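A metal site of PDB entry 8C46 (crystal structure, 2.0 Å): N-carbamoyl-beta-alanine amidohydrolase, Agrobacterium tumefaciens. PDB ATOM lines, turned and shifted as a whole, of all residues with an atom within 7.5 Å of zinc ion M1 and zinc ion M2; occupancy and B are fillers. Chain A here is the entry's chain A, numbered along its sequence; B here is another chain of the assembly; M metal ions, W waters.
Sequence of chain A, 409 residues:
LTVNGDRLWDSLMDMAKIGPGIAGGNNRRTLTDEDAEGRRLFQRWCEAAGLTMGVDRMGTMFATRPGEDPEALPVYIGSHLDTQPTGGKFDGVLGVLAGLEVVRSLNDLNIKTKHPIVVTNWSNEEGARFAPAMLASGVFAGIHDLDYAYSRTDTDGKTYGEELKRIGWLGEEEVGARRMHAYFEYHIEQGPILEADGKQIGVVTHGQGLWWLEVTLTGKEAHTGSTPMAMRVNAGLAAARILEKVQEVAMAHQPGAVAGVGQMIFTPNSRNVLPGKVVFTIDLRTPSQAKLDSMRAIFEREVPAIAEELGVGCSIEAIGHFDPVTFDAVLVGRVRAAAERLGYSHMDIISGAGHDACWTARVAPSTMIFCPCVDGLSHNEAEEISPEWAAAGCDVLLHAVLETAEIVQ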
ATOM      1  N   SER A  79       5.381  -1.205 -16.387  1.00  0.00           N
ATOM      2  CA  SER A  79       6.799  -0.826 -16.292  1.00  0.00           C
ATOM      3  C   SER A  79       6.932   0.430 -15.417  1.00  0.00           C
ATOM      4  O   SER A  79       6.240   0.498 -14.391  1.00  0.00           O
ATOM      5  CB  SER A  79       7.425  -0.701 -17.649  1.00  0.00           C
ATOM      6  OG  SER A  79       8.822  -0.902 -17.586  1.00  0.00           O
ATOM      7  N   HIS A  80       7.793   1.402 -15.794  1.00  0.00           N
ATOM      8  CA  HIS A  80       8.094   2.580 -14.991  1.00  0.00           C
ATOM      9  C   HIS A  80       8.320   3.781 -15.893  1.00  0.00           C
ATOM     10  O   HIS A  80       8.931   3.657 -16.947  1.00  0.00           O
ATOM     11  CB  HIS A  80       9.332   2.370 -14.102  1.00  0.00           C
ATOM     12  CG  HIS A  80      10.567   2.063 -14.846  1.00  0.00           C
ATOM     13  ND1 HIS A  80      11.436   3.046 -15.280  1.00  0.00           N
ATOM     14  CD2 HIS A  80      11.059   0.909 -15.337  1.00  0.00           C
ATOM     15  CE1 HIS A  80      12.431   2.526 -15.948  1.00  0.00           C
ATOM     16  NE2 HIS A  80      12.238   1.250 -15.993  1.00  0.00           N
ATOM     17  N   ASP A  82       9.872   6.565 -14.422  1.00  0.00           N
ATOM     18  CA  ASP A  82      11.035   7.224 -13.850  1.00  0.00           C
ATOM     19  C   ASP A  82      12.291   6.794 -14.629  1.00  0.00           C
ATOM     20  O   ASP A  82      12.372   5.662 -15.132  1.00  0.00           O
ATOM     21  CB  ASP A  82      11.157   6.980 -12.335  1.00  0.00           C
ATOM     22  CG  ASP A  82      11.622   5.576 -11.975  1.00  0.00           C
ATOM     23  OD1 ASP A  82      10.776   4.613 -12.124  1.00  0.00           O
ATOM     24  OD2 ASP A  82      12.815   5.442 -11.590  1.00  0.00           O
ATOM     25  N   THR A  83      13.251   7.714 -14.703  1.00  0.00           N
ATOM     26  CA  THR A  83      14.442   7.523 -15.518  1.00  0.00           C
ATOM     27  C   THR A  83      15.687   7.718 -14.652  1.00  0.00           C
ATOM     28  O   THR A  83      15.648   8.211 -13.525  1.00  0.00           O
ATOM     29  CB  THR A  83      14.459   8.504 -16.702  1.00  0.00           C
ATOM     30  OG1 THR A  83      14.733   9.851 -16.277  1.00  0.00           O
ATOM     31  CG2 THR A  83      13.153   8.498 -17.470  1.00  0.00           C
ATOM     32  N   GLN A  84      16.801   7.253 -15.211  1.00  0.00           N
ATOM     33  CA  GLN A  84      18.127   7.630 -14.780  1.00  0.00           C
ATOM     34  C   GLN A  84      18.354   9.130 -15.002  1.00  0.00           C
ATOM     35  O   GLN A  84      17.696   9.759 -15.846  1.00  0.00           O
ATOM     36  CB  GLN A  84      19.103   6.785 -15.592  1.00  0.00           C
ATOM     37  CG  GLN A  84      19.092   5.298 -15.196  1.00  0.00           C
ATOM     38  CD  GLN A  84      19.818   5.061 -13.883  1.00  0.00           C
ATOM     39  OE1 GLN A  84      20.786   5.765 -13.586  1.00  0.00           O
ATOM     40  NE2 GLN A  84      19.331   4.116 -13.085  1.00  0.00           N
ATOM     41  N   PHE A  90      13.296   5.390 -23.606  1.00  0.00           N
ATOM     42  CA  PHE A  90      12.577   4.148 -23.904  1.00  0.00           C
ATOM     43  C   PHE A  90      12.596   3.177 -22.717  1.00  0.00           C
ATOM     44  O   PHE A  90      11.622   2.438 -22.502  1.00  0.00           O
ATOM     45  CB  PHE A  90      13.140   3.491 -25.161  1.00  0.00           C
ATOM     46  CG  PHE A  90      13.152   4.399 -26.359  1.00  0.00           C
ATOM     47  CD1 PHE A  90      11.945   4.821 -26.910  1.00  0.00           C
ATOM     48  CD2 PHE A  90      14.345   4.906 -26.881  1.00  0.00           C
ATOM     49  CE1 PHE A  90      11.929   5.687 -27.988  1.00  0.00           C
ATOM     50  CE2 PHE A  90      14.312   5.772 -27.956  1.00  0.00           C
ATOM     51  CZ  PHE A  90      13.118   6.135 -28.529  1.00  0.00           C
ATOM     52  N   ASP A  91      13.687   3.202 -21.941  1.00  0.00           N
ATOM     53  CA  ASP A  91      13.755   2.417 -20.738  1.00  0.00           C
ATOM     54  C   ASP A  91      12.562   2.731 -19.846  1.00  0.00           C
ATOM     55  O   ASP A  91      12.359   3.915 -19.488  1.00  0.00           O
ATOM     56  CB  ASP A  91      15.056   2.741 -20.021  1.00  0.00           C
ATOM     57  CG  ASP A  91      15.223   2.001 -18.715  1.00  0.00           C
ATOM     58  OD1 ASP A  91      14.287   1.253 -18.267  1.00  0.00           O
ATOM     59  OD2 ASP A  91      16.323   2.133 -18.196  1.00  0.00           O
ATOM     60  N   GLY A  92      11.791   1.684 -19.520  1.00  0.00           N
ATOM     61  CA  GLY A  92      10.623   1.866 -18.667  1.00  0.00           C
ATOM     62  C   GLY A  92       9.411   2.406 -19.419  1.00  0.00           C
ATOM     63  O   GLY A  92       8.325   1.818 -19.412  1.00  0.00           O
ATOM     64  N   VAL A  93       9.592   3.555 -20.077  1.00  0.00           N
ATOM     65  CA  VAL A  93       8.520   4.286 -20.719  1.00  0.00           C
ATOM     66  C   VAL A  93       7.852   3.402 -21.770  1.00  0.00           C
ATOM     67  O   VAL A  93       6.637   3.463 -21.955  1.00  0.00           O
ATOM     68  CB  VAL A  93       9.009   5.613 -21.316  1.00  0.00           C
ATOM     69  CG1 VAL A  93       7.878   6.397 -21.930  1.00  0.00           C
ATOM     70  CG2 VAL A  93       9.752   6.468 -20.333  1.00  0.00           C
ATOM     71  N   GLU A 125      11.465   2.604 -10.134  1.00  0.00           N
ATOM     72  CA  GLU A 125      12.128   1.410 -10.580  1.00  0.00           C
ATOM     73  C   GLU A 125      13.658   1.610 -10.625  1.00  0.00           C
ATOM     74  O   GLU A 125      14.342   0.620 -10.319  1.00  0.00           O
ATOM     75  CB  GLU A 125      11.670   0.944 -11.960  1.00  0.00           C
ATOM     76  CG  GLU A 125      12.209  -0.444 -12.265  1.00  0.00           C
ATOM     77  CD  GLU A 125      13.631  -0.511 -12.799  1.00  0.00           C
ATOM     78  OE1 GLU A 125      14.081   0.486 -13.399  1.00  0.00           O
ATOM     79  OE2 GLU A 125      14.275  -1.585 -12.584  1.00  0.00           O
ATOM     80  N   GLU A 126      14.138   2.801 -11.073  1.00  0.00           N
ATOM     81  CA  GLU A 126      15.534   2.935 -11.476  1.00  0.00           C
ATOM     82  C   GLU A 126      16.549   2.806 -10.310  1.00  0.00           C
ATOM     83  O   GLU A 126      17.653   2.255 -10.484  1.00  0.00           O
ATOM     84  CB  GLU A 126      15.749   4.222 -12.279  1.00  0.00           C
ATOM     85  CG  GLU A 126      15.209   4.141 -13.685  1.00  0.00           C
ATOM     86  CD  GLU A 126      15.956   3.264 -14.679  1.00  0.00           C
ATOM     87  OE1 GLU A 126      16.874   2.474 -14.332  1.00  0.00           O
ATOM     88  OE2 GLU A 126      15.623   3.340 -15.881  1.00  0.00           O
ATOM     89  N   GLY A 127      16.186   3.308  -9.131  1.00  0.00           N
ATOM     90  CA  GLY A 127      17.063   3.249  -7.966  1.00  0.00           C
ATOM     91  C   GLY A 127      18.285   4.166  -8.118  1.00  0.00           C
ATOM     92  O   GLY A 127      19.330   3.944  -7.516  1.00  0.00           O
ATOM     93  N   GLU A 185       5.614  -7.470 -18.649  1.00  0.00           N
ATOM     94  CA  GLU A 185       6.392  -6.248 -18.853  1.00  0.00           C
ATOM     95  C   GLU A 185       7.143  -6.273 -20.179  1.00  0.00           C
ATOM     96  O   GLU A 185       7.904  -7.211 -20.450  1.00  0.00           O
ATOM     97  CB  GLU A 185       7.288  -5.997 -17.658  1.00  0.00           C
ATOM     98  CG  GLU A 185       8.249  -4.822 -17.841  1.00  0.00           C
ATOM     99  CD  GLU A 185       8.830  -4.290 -16.540  1.00  0.00           C
ATOM    100  OE1 GLU A 185       8.511  -4.834 -15.454  1.00  0.00           O
ATOM    101  OE2 GLU A 185       9.498  -3.230 -16.642  1.00  0.00           O
ATOM    102  N   HIS A 187       9.932  -4.302 -22.326  1.00  0.00           N
ATOM    103  CA  HIS A 187      11.080  -3.422 -22.029  1.00  0.00           C
ATOM    104  C   HIS A 187      12.146  -3.547 -23.125  1.00  0.00           C
ATOM    105  O   HIS A 187      12.227  -4.556 -23.793  1.00  0.00           O
ATOM    106  CB  HIS A 187      11.620  -3.784 -20.654  1.00  0.00           C
ATOM    107  CG  HIS A 187      12.529  -2.821 -20.003  1.00  0.00           C
ATOM    108  ND1 HIS A 187      13.786  -2.424 -20.433  1.00  0.00           N
ATOM    109  CD2 HIS A 187      12.244  -2.131 -18.871  1.00  0.00           C
ATOM    110  CE1 HIS A 187      14.238  -1.515 -19.598  1.00  0.00           C
ATOM    111  NE2 HIS A 187      13.329  -1.324 -18.630  1.00  0.00           N
ATOM    112  N   ILE A 188      13.004  -2.512 -23.269  1.00  0.00           N
ATOM    113  CA  ILE A 188      14.191  -2.633 -24.121  1.00  0.00           C
ATOM    114  C   ILE A 188      15.171  -3.650 -23.501  1.00  0.00           C
ATOM    115  O   ILE A 188      15.235  -3.817 -22.283  1.00  0.00           O
ATOM    116  CB  ILE A 188      14.834  -1.257 -24.390  1.00  0.00           C
ATOM    117  CG1 ILE A 188      15.432  -0.610 -23.149  1.00  0.00           C
ATOM    118  CG2 ILE A 188      13.812  -0.319 -25.041  1.00  0.00           C
ATOM    119  CD1 ILE A 188      16.324   0.538 -23.429  1.00  0.00           C
ATOM    120  N   GLN A 190      18.345  -3.472 -23.151  1.00  0.00           N
ATOM    121  CA  GLN A 190      19.430  -2.792 -22.446  1.00  0.00           C
ATOM    122  C   GLN A 190      20.754  -3.503 -22.716  1.00  0.00           C
ATOM    123  O   GLN A 190      21.734  -3.310 -22.005  1.00  0.00           O
ATOM    124  CB  GLN A 190      19.180  -2.660 -20.936  1.00  0.00           C
ATOM    125  CG  GLN A 190      17.919  -1.897 -20.541  1.00  0.00           C
ATOM    126  CD  GLN A 190      17.799  -1.913 -19.037  1.00  0.00           C
ATOM    127  OE1 GLN A 190      17.658  -2.971 -18.426  1.00  0.00           O
ATOM    128  NE2 GLN A 190      17.778  -0.740 -18.418  1.00  0.00           N
ATOM    129  N   ALA A 353      19.307  -7.356 -16.801  1.00  0.00           N
ATOM    130  CA  ALA A 353      18.994  -6.505 -15.654  1.00  0.00           C
ATOM    131  C   ALA A 353      17.815  -7.034 -14.825  1.00  0.00           C
ATOM    132  O   ALA A 353      17.066  -7.908 -15.227  1.00  0.00           O
ATOM    133  CB  ALA A 353      18.681  -5.092 -16.087  1.00  0.00           C
ATOM    134  N   GLY A 354      17.638  -6.454 -13.630  1.00  0.00           N
ATOM    135  CA  GLY A 354      16.419  -6.599 -12.856  1.00  0.00           C
ATOM    136  C   GLY A 354      15.403  -5.587 -13.376  1.00  0.00           C
ATOM    137  O   GLY A 354      15.773  -4.595 -13.964  1.00  0.00           O
ATOM    138  N   HIS A 355      14.129  -5.959 -13.267  1.00  0.00           N
ATOM    139  CA  HIS A 355      12.947  -5.164 -13.579  1.00  0.00           C
ATOM    140  C   HIS A 355      11.910  -5.512 -12.517  1.00  0.00           C
ATOM    141  O   HIS A 355      11.987  -6.567 -11.866  1.00  0.00           O
ATOM    142  CB  HIS A 355      12.409  -5.481 -14.974  1.00  0.00           C
ATOM    143  CG  HIS A 355      13.499  -5.433 -16.025  1.00  0.00           C
ATOM    144  ND1 HIS A 355      13.935  -4.270 -16.596  1.00  0.00           N
ATOM    145  CD2 HIS A 355      14.292  -6.480 -16.557  1.00  0.00           C
ATOM    146  CE1 HIS A 355      14.884  -4.585 -17.515  1.00  0.00           C
ATOM    147  NE2 HIS A 355      15.158  -5.914 -17.446  1.00  0.00           N
ATOM    148  N   ASP A 356      10.899  -4.640 -12.439  1.00  0.00           N
ATOM    149  CA  ASP A 356       9.742  -4.851 -11.600  1.00  0.00           C
ATOM    150  C   ASP A 356       9.141  -6.246 -11.831  1.00  0.00           C
ATOM    151  O   ASP A 356       8.666  -6.856 -10.902  1.00  0.00           O
ATOM    152  CB  ASP A 356       8.690  -3.748 -11.848  1.00  0.00           C
ATOM    153  CG  ASP A 356       9.184  -2.353 -11.520  1.00  0.00           C
ATOM    154  OD1 ASP A 356       9.634  -2.196 -10.392  1.00  0.00           O
ATOM    155  OD2 ASP A 356       9.225  -1.453 -12.462  1.00  0.00           O
ATOM    156  N   MET A 368       8.333 -11.283 -19.367  1.00  0.00           N
ATOM    157  CA  MET A 368       8.764 -10.077 -20.052  1.00  0.00           C
ATOM    158  C   MET A 368       8.873 -10.277 -21.555  1.00  0.00           C
ATOM    159  O   MET A 368       9.083 -11.373 -22.027  1.00  0.00           O
ATOM    160  CB  MET A 368      10.129  -9.628 -19.569  1.00  0.00           C
ATOM    161  CG  MET A 368      10.131  -9.313 -18.091  1.00  0.00           C
ATOM    162  SD  MET A 368      11.625  -8.467 -17.635  1.00  0.00           S
ATOM    163  CE  MET A 368      11.142  -6.790 -18.003  1.00  0.00           C
ATOM    164  N   SER A 378      21.866   1.646 -22.954  1.00  0.00           N
ATOM    165  CA  SER A 378      20.788   2.055 -22.054  1.00  0.00           C
ATOM    166  C   SER A 378      21.405   2.825 -20.893  1.00  0.00           C
ATOM    167  O   SER A 378      22.611   2.944 -20.839  1.00  0.00           O
ATOM    168  CB  SER A 378      19.934   0.869 -21.561  1.00  0.00           C
ATOM    169  OG  SER A 378      18.780   1.337 -20.856  1.00  0.00           O
ATOM    170  N   HIS A 379      20.554   3.466 -20.077  1.00  0.00           N
ATOM    171  CA  HIS A 379      20.975   4.316 -18.950  1.00  0.00           C
ATOM    172  C   HIS A 379      21.861   5.464 -19.448  1.00  0.00           C
ATOM    173  O   HIS A 379      22.787   5.871 -18.744  1.00  0.00           O
ATOM    174  CB  HIS A 379      21.672   3.520 -17.833  1.00  0.00           C
ATOM    175  CG  HIS A 379      20.752   2.669 -17.050  1.00  0.00           C
ATOM    176  ND1 HIS A 379      21.010   2.322 -15.759  1.00  0.00           N
ATOM    177  CD2 HIS A 379      19.480   2.228 -17.320  1.00  0.00           C
ATOM    178  CE1 HIS A 379      19.977   1.606 -15.297  1.00  0.00           C
ATOM    179  NE2 HIS A 379      19.041   1.569 -16.231  1.00  0.00           N
ATOM    180  N   GLU A 383      20.294   6.253 -25.845  1.00  0.00           N
ATOM    181  CA  GLU A 383      19.543   5.003 -25.899  1.00  0.00           C
ATOM    182  C   GLU A 383      18.491   5.101 -27.000  1.00  0.00           C
ATOM    183  O   GLU A 383      17.741   6.097 -27.062  1.00  0.00           O
ATOM    184  CB  GLU A 383      18.923   4.753 -24.518  1.00  0.00           C
ATOM    185  CG  GLU A 383      17.889   3.634 -24.472  1.00  0.00           C
ATOM    186  CD  GLU A 383      17.065   3.717 -23.210  1.00  0.00           C
ATOM    187  OE1 GLU A 383      17.564   3.263 -22.147  1.00  0.00           O
ATOM    188  OE2 GLU A 383      15.957   4.317 -23.289  1.00  0.00           O
ATOM    189  N   HIS B 223      25.348  -1.464 -19.461  1.00  0.00           N
ATOM    190  CA  HIS B 223      24.759  -2.031 -18.265  1.00  0.00           C
ATOM    191  C   HIS B 223      25.584  -3.273 -17.878  1.00  0.00           C
ATOM    192  O   HIS B 223      25.863  -4.124 -18.691  1.00  0.00           O
ATOM    193  CB  HIS B 223      23.262  -2.281 -18.548  1.00  0.00           C
ATOM    194  CG  HIS B 223      22.457  -2.462 -17.343  1.00  0.00           C
ATOM    195  ND1 HIS B 223      22.574  -3.584 -16.544  1.00  0.00           N
ATOM    196  CD2 HIS B 223      21.539  -1.650 -16.788  1.00  0.00           C
ATOM    197  CE1 HIS B 223      21.818  -3.419 -15.488  1.00  0.00           C
ATOM    198  NE2 HIS B 223      21.124  -2.277 -15.631  1.00  0.00           N
ATOM    199  N   ASN B 272      25.854  -0.050 -11.812  1.00  0.00           N
ATOM    200  CA  ASN B 272      25.330  -0.959 -12.840  1.00  0.00           C
ATOM    201  C   ASN B 272      25.676  -0.481 -14.258  1.00  0.00           C
ATOM    202  O   ASN B 272      25.029  -0.887 -15.223  1.00  0.00           O
ATOM    203  CB  ASN B 272      23.865  -1.213 -12.634  1.00  0.00           C
ATOM    204  CG  ASN B 272      23.069   0.075 -12.666  1.00  0.00           C
ATOM    205  OD1 ASN B 272      23.630   1.154 -12.813  1.00  0.00           O
ATOM    206  ND2 ASN B 272      21.786   0.008 -12.450  1.00  0.00           N
HETATM  207 ZN    ZN M   1      13.675  -0.137 -16.788  1.00  0.00          ZN
HETATM  208 ZN    ZN M   2      16.605   1.461 -16.303  1.00  0.00          ZN
HETATM  209  O   HOH W   1      15.491  -0.372 -16.046  1.00  0.00           O
HETATM  210  O   HOH W   2      12.926  -1.924 -15.587  1.00  0.00           O
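Zinc ion M1 is bound by water W1 (2.0 Å), OD1 of Asp 91 (2.1 Å), NE2 of His 80 (2.1 Å), NE2 of His 187 (2.2 Å) and water W2 (2.3 Å).
Zinc ion M2 is bound by OD2 of Asp 91, water W1, OE2 of Glu 126, OE1 of Glu 126 and NE2 of His 379.
OG of Ser 79 lies close to O of Gly 92 (3.3 Å).
The backbone NH (N) of Gly 92 sits close to a ring nitrogen (NE2) of His 187, 3.5 Å away.
OD1 of Asp 82 sits at hydrogen-bond distance from N of Glu 125 (2.9 Å).
OE1 of Glu 125 sits close to NE2 of His 80 (3.3 Å).
The backbone NH of Asp 91 lies within hydrogen-bond range of the side-chain carboxylate of Glu 383 (2.9 Å).
The side-chain carboxylate of Glu 126 lies close to the side-chain amide nitrogen of Gln 84.
The backbone NH of Glu 126 sits at hydrogen-bond distance from the side-chain carboxylate of Asp 82, 3.0 Å away.
The side-chain amide nitrogen of Gln 190 lies close to a ring nitrogen (NE2) of His 379.
Residues that only touch zinc ion M1: Gly 92 and Glu 125.
Water W2 lies within hydrogen-bond range of ND1 of His 355 and OE2 of Glu 125.
Water W1 lies within hydrogen-bond range of OE1 of Glu 125 (3.1 Å) and NE2 of Gln 190 (3.3 Å).
Glu 125 touches zinc ion M2 (OE1 to ZN, 3.97 Å).
NE2 of Gln 190 touches zinc ion M2 (3.3 Å).
Of the 26 residues printed, 5 come within 4 Å of zinc ion M2.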
